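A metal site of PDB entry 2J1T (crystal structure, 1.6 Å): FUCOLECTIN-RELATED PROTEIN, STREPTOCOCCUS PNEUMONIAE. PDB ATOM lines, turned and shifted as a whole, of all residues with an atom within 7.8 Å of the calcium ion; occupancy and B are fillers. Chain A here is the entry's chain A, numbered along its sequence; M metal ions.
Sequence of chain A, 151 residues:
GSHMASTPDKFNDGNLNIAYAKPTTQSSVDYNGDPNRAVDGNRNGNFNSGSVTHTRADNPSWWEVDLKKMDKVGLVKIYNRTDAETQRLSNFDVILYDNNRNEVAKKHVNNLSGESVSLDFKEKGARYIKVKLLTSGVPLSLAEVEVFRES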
ATOM      1  N   PRO A  35     -28.699   6.799  36.673  1.00  0.00           N
ATOM      2  CA  PRO A  35     -27.752   5.761  36.253  1.00  0.00           C
ATOM      3  C   PRO A  35     -28.386   4.546  35.651  1.00  0.00           C
ATOM      4  O   PRO A  35     -27.740   3.830  34.856  1.00  0.00           O
ATOM      5  CB  PRO A  35     -27.005   5.446  37.574  1.00  0.00           C
ATOM      6  CG  PRO A  35     -27.924   5.884  38.640  1.00  0.00           C
ATOM      7  CD  PRO A  35     -28.657   7.079  38.094  1.00  0.00           C
ATOM      8  N   ASN A  36     -29.662   4.309  35.969  1.00  0.00           N
ATOM      9  CA  ASN A  36     -30.337   3.146  35.344  1.00  0.00           C
ATOM     10  C   ASN A  36     -30.542   3.265  33.853  1.00  0.00           C
ATOM     11  O   ASN A  36     -30.842   2.280  33.153  1.00  0.00           O
ATOM     12  CB  ASN A  36     -31.651   2.811  36.088  1.00  0.00           C
ATOM     13  CG  ASN A  36     -32.768   3.823  35.865  1.00  0.00           C
ATOM     14  OD1 ASN A  36     -33.961   3.487  36.014  1.00  0.00           O
ATOM     15  ND2 ASN A  36     -32.418   5.030  35.617  1.00  0.00           N
ATOM     16  N   ARG A  37     -30.340   4.459  33.299  1.00  0.00           N
ATOM     17  CA  ARG A  37     -30.456   4.611  31.845  1.00  0.00           C
ATOM     18  C   ARG A  37     -29.393   3.849  31.051  1.00  0.00           C
ATOM     19  O   ARG A  37     -29.587   3.556  29.882  1.00  0.00           O
ATOM     20  CB  ARG A  37     -30.479   6.084  31.459  1.00  0.00           C
ATOM     21  CG  ARG A  37     -31.695   6.849  32.018  1.00  0.00           C
ATOM     22  CD  ARG A  37     -31.660   8.333  31.758  1.00  0.00           C
ATOM     23  NE  ARG A  37     -32.875   8.886  32.408  1.00  0.00           N
ATOM     24  CZ  ARG A  37     -33.490  10.001  32.132  1.00  0.00           C
ATOM     25  NH1 ARG A  37     -34.607  10.307  32.845  1.00  0.00           N
ATOM     26  NH2 ARG A  37     -33.013  10.836  31.220  1.00  0.00           N
ATOM     27  N   ALA A  38     -28.275   3.486  31.706  1.00  0.00           N
ATOM     28  CA  ALA A  38     -27.252   2.717  31.041  1.00  0.00           C
ATOM     29  C   ALA A  38     -27.490   1.231  31.066  1.00  0.00           C
ATOM     30  O   ALA A  38     -26.718   0.478  30.508  1.00  0.00           O
ATOM     31  CB  ALA A  38     -25.865   3.087  31.605  1.00  0.00           C
ATOM     32  N   VAL A  39     -28.567   0.792  31.731  1.00  0.00           N
ATOM     33  CA  VAL A  39     -28.932  -0.613  31.746  1.00  0.00           C
ATOM     34  C   VAL A  39     -30.401  -0.798  31.378  1.00  0.00           C
ATOM     35  O   VAL A  39     -31.024  -1.786  31.787  1.00  0.00           O
ATOM     36  CB  VAL A  39     -28.556  -1.330  33.093  1.00  0.00           C
ATOM     37  CG1 VAL A  39     -27.044  -1.300  33.302  1.00  0.00           C
ATOM     38  CG2 VAL A  39     -29.318  -0.767  34.305  1.00  0.00           C
ATOM     39  N   ASP A  40     -30.904   0.111  30.536  1.00  0.00           N
ATOM     40  CA  ASP A  40     -32.301   0.051  30.165  1.00  0.00           C
ATOM     41  C   ASP A  40     -32.633  -0.687  28.881  1.00  0.00           C
ATOM     42  O   ASP A  40     -33.817  -0.742  28.498  1.00  0.00           O
ATOM     43  CB  ASP A  40     -32.905   1.458  30.170  1.00  0.00           C
ATOM     44  CG  ASP A  40     -32.419   2.343  29.077  1.00  0.00           C
ATOM     45  OD1 ASP A  40     -31.530   1.989  28.295  1.00  0.00           O
ATOM     46  OD2 ASP A  40     -32.896   3.513  28.939  1.00  0.00           O
ATOM     47  N   GLY A  41     -31.646  -1.352  28.302  1.00  0.00           N
ATOM     48  CA  GLY A  41     -31.789  -2.158  27.076  1.00  0.00           C
ATOM     49  C   GLY A  41     -31.726  -1.275  25.857  1.00  0.00           C
ATOM     50  O   GLY A  41     -31.892  -1.780  24.776  1.00  0.00           O
ATOM     51  N   ASN A  42     -31.441   0.016  26.011  1.00  0.00           N
ATOM     52  CA  ASN A  42     -31.549   0.957  24.874  1.00  0.00           C
ATOM     53  C   ASN A  42     -30.189   1.560  24.623  1.00  0.00           C
ATOM     54  O   ASN A  42     -29.660   2.304  25.453  1.00  0.00           O
ATOM     55  CB  ASN A  42     -32.578   2.037  25.172  1.00  0.00           C
ATOM     56  CG  ASN A  42     -32.792   2.995  23.994  1.00  0.00           C
ATOM     57  OD1 ASN A  42     -32.280   2.775  22.897  1.00  0.00           O
ATOM     58  ND2 ASN A  42     -33.673   4.014  24.207  1.00  0.00           N
ATOM     59  N   ARG A  43     -29.633   1.271  23.449  1.00  0.00           N
ATOM     60  CA  ARG A  43     -28.312   1.784  23.085  1.00  0.00           C
ATOM     61  C   ARG A  43     -28.323   3.208  22.510  1.00  0.00           C
ATOM     62  O   ARG A  43     -27.230   3.771  22.222  1.00  0.00           O
ATOM     63  CB  ARG A  43     -27.635   0.873  22.081  1.00  0.00           C
ATOM     64  CG  ARG A  43     -27.319  -0.509  22.603  1.00  0.00           C
ATOM     65  CD  ARG A  43     -26.890  -1.428  21.501  1.00  0.00           C
ATOM     66  NE  ARG A  43     -26.549  -2.756  21.962  1.00  0.00           N
ATOM     67  CZ  ARG A  43     -26.226  -3.764  21.159  1.00  0.00           C
ATOM     68  NH1 ARG A  43     -25.911  -4.941  21.686  1.00  0.00           N
ATOM     69  NH2 ARG A  43     -26.153  -3.570  19.851  1.00  0.00           N
ATOM     70  N   ASN A  44     -29.501   3.789  22.327  1.00  0.00           N
ATOM     71  CA  ASN A  44     -29.621   5.109  21.706  1.00  0.00           C
ATOM     72  C   ASN A  44     -28.755   6.084  22.520  1.00  0.00           C
ATOM     73  O   ASN A  44     -28.870   6.153  23.768  1.00  0.00           O
ATOM     74  CB  ASN A  44     -31.108   5.535  21.673  1.00  0.00           C
ATOM     75  CG  ASN A  44     -31.404   6.763  20.826  1.00  0.00           C
ATOM     76  OD1 ASN A  44     -32.614   7.061  20.529  1.00  0.00           O
ATOM     77  ND2 ASN A  44     -30.389   7.508  20.498  1.00  0.00           N
ATOM     78  N   GLY A  45     -27.857   6.790  21.839  1.00  0.00           N
ATOM     79  CA  GLY A  45     -26.936   7.718  22.460  1.00  0.00           C
ATOM     80  C   GLY A  45     -27.342   9.153  22.408  1.00  0.00           C
ATOM     81  O   GLY A  45     -26.588  10.019  22.881  1.00  0.00           O
ATOM     82  N   SER A  49     -33.240  11.418  24.007  1.00  0.00           N
ATOM     83  CA  SER A  49     -33.983  10.148  23.906  1.00  0.00           C
ATOM     84  C   SER A  49     -34.354   9.579  25.266  1.00  0.00           C
ATOM     85  O   SER A  49     -35.262   8.746  25.364  1.00  0.00           O
ATOM     86  CB  SER A  49     -33.142   9.051  23.162  1.00  0.00           C
ATOM     87  OG  SER A  49     -32.044   8.491  23.981  1.00  0.00           O
ATOM     88  N   GLY A  50     -33.670  10.035  26.314  1.00  0.00           N
ATOM     89  CA  GLY A  50     -33.847   9.494  27.641  1.00  0.00           C
ATOM     90  C   GLY A  50     -33.086   8.257  28.010  1.00  0.00           C
ATOM     91  O   GLY A  50     -33.311   7.664  29.072  1.00  0.00           O
ATOM     92  N   SER A  51     -32.246   7.804  27.096  1.00  0.00           N
ATOM     93  CA  SER A  51     -31.476   6.547  27.158  1.00  0.00           C
ATOM     94  C   SER A  51     -30.122   6.705  27.824  1.00  0.00           C
ATOM     95  O   SER A  51     -29.434   5.706  27.992  1.00  0.00           O
ATOM     96  CB  SER A  51     -31.211   6.040  25.713  1.00  0.00           C
ATOM     97  OG  SER A  51     -30.449   4.791  25.658  1.00  0.00           O
ATOM     98  N   VAL A  52     -29.711   7.936  28.102  1.00  0.00           N
ATOM     99  CA  VAL A  52     -28.306   8.250  28.403  1.00  0.00           C
ATOM    100  C   VAL A  52     -28.193   8.820  29.809  1.00  0.00           C
ATOM    101  O   VAL A  52     -28.982   9.704  30.179  1.00  0.00           O
ATOM    102  CB  VAL A  52     -27.746   9.240  27.367  1.00  0.00           C
ATOM    103  CG1 VAL A  52     -26.198   9.533  27.552  1.00  0.00           C
ATOM    104  CG2 VAL A  52     -27.992   8.762  25.956  1.00  0.00           C
ATOM    105  N   THR A  53     -27.206   8.357  30.572  1.00  0.00           N
ATOM    106  CA  THR A  53     -26.950   8.883  31.910  1.00  0.00           C
ATOM    107  C   THR A  53     -26.263  10.231  31.834  1.00  0.00           C
ATOM    108  O   THR A  53     -25.816  10.656  30.781  1.00  0.00           O
ATOM    109  CB  THR A  53     -26.088   7.926  32.706  1.00  0.00           C
ATOM    110  OG1 THR A  53     -24.752   7.912  32.166  1.00  0.00           O
ATOM    111  CG2 THR A  53     -26.624   6.451  32.692  1.00  0.00           C
ATOM    112  N   TYR A  79     -21.336   2.046  25.402  1.00  0.00           N
ATOM    113  CA  TYR A  79     -21.884   2.851  24.300  1.00  0.00           C
ATOM    114  C   TYR A  79     -21.921   4.305  24.764  1.00  0.00           C
ATOM    115  O   TYR A  79     -22.444   4.628  25.822  1.00  0.00           O
ATOM    116  CB  TYR A  79     -23.272   2.339  23.953  1.00  0.00           C
ATOM    117  CG  TYR A  79     -23.291   0.917  23.445  1.00  0.00           C
ATOM    118  CD1 TYR A  79     -23.325   0.630  22.087  1.00  0.00           C
ATOM    119  CD2 TYR A  79     -23.262  -0.150  24.329  1.00  0.00           C
ATOM    120  CE1 TYR A  79     -23.302  -0.666  21.616  1.00  0.00           C
ATOM    121  CE2 TYR A  79     -23.252  -1.456  23.863  1.00  0.00           C
ATOM    122  CZ  TYR A  79     -23.291  -1.702  22.528  1.00  0.00           C
ATOM    123  OH  TYR A  79     -23.278  -3.031  22.086  1.00  0.00           O
ATOM    124  N   LEU A 142     -23.263   7.873  29.730  1.00  0.00           N
ATOM    125  CA  LEU A 142     -23.186   6.592  29.033  1.00  0.00           C
ATOM    126  C   LEU A 142     -24.571   6.258  28.447  1.00  0.00           C
ATOM    127  O   LEU A 142     -25.590   6.358  29.130  1.00  0.00           O
ATOM    128  CB  LEU A 142     -22.822   5.493  30.058  1.00  0.00           C
ATOM    129  CG  LEU A 142     -21.478   5.714  30.778  1.00  0.00           C
ATOM    130  CD1 LEU A 142     -21.342   4.835  31.987  1.00  0.00           C
ATOM    131  CD2 LEU A 142     -20.344   5.486  29.787  1.00  0.00           C
ATOM    132  N   ALA A 143     -24.599   5.900  27.154  1.00  0.00           N
ATOM    133  CA  ALA A 143     -25.811   5.431  26.540  1.00  0.00           C
ATOM    134  C   ALA A 143     -26.244   4.053  27.064  1.00  0.00           C
ATOM    135  O   ALA A 143     -27.461   3.779  27.268  1.00  0.00           O
ATOM    136  CB  ALA A 143     -25.648   5.442  25.041  1.00  0.00           C
ATOM    137  N   GLU A 144     -25.266   3.175  27.250  1.00  0.00           N
ATOM    138  CA  GLU A 144     -25.575   1.822  27.697  1.00  0.00           C
ATOM    139  C   GLU A 144     -24.233   1.143  28.060  1.00  0.00           C
ATOM    140  O   GLU A 144     -23.186   1.412  27.435  1.00  0.00           O
ATOM    141  CB  GLU A 144     -26.258   1.028  26.606  1.00  0.00           C
ATOM    142  CG  GLU A 144     -26.936  -0.223  27.102  1.00  0.00           C
ATOM    143  CD  GLU A 144     -28.245  -0.058  27.831  1.00  0.00           C
ATOM    144  OE1 GLU A 144     -28.747   1.102  28.037  1.00  0.00           O
ATOM    145  OE2 GLU A 144     -28.734  -1.149  28.249  1.00  0.00           O
ATOM    146  N   VAL A 145     -24.273   0.320  29.093  1.00  0.00           N
ATOM    147  CA  VAL A 145     -23.173  -0.596  29.432  1.00  0.00           C
ATOM    148  C   VAL A 145     -23.720  -1.999  29.468  1.00  0.00           C
ATOM    149  O   VAL A 145     -24.652  -2.279  30.206  1.00  0.00           O
ATOM    150  CB  VAL A 145     -22.517  -0.223  30.776  1.00  0.00           C
ATOM    151  CG1 VAL A 145     -21.407  -1.217  31.161  1.00  0.00           C
ATOM    152  CG2 VAL A 145     -21.979   1.220  30.733  1.00  0.00           C
HETATM  153 CA    CA M   1     -29.576   3.239  27.620  1.00  0.00          CA
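The backbone NH (N) of Gly 41 is in hydrogen-bond range of the side-chain carboxylate (OE2) of Glu 144, 2.9 Å away.
The backbone carbonyl oxygen (O) of Tyr 79 is in hydrogen-bond range of the backbone NH (N) of Ala 143 (2.8 Å).
The side-chain hydroxyl (OG) of Ser 49 sits close to the backbone NH (N) of Ser 51, 3.2 Å away.
The side-chain amide oxygen (OD1) of Asn 42 is in hydrogen-bond range of the backbone NH (N) of Asn 44, 3.0 Å away.
The backbone NH of Tyr 79 lies within hydrogen-bond range of the backbone carbonyl oxygen of Glu 144 (2.8 Å).
O of Asn 44 lies close to OG of Ser 51 (2.8 Å).
The calcium ion is bound by O of Ala 143 (2.2 Å), O of Arg 37 (2.3 Å), OE1 of Glu 144 (2.3 Å), O of Asn 42 (2.4 Å), OD1 of Asp 40 (2.4 Å), O of Ser 51 (2.5 Å) and OG of Ser 51 (2.6 Å).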
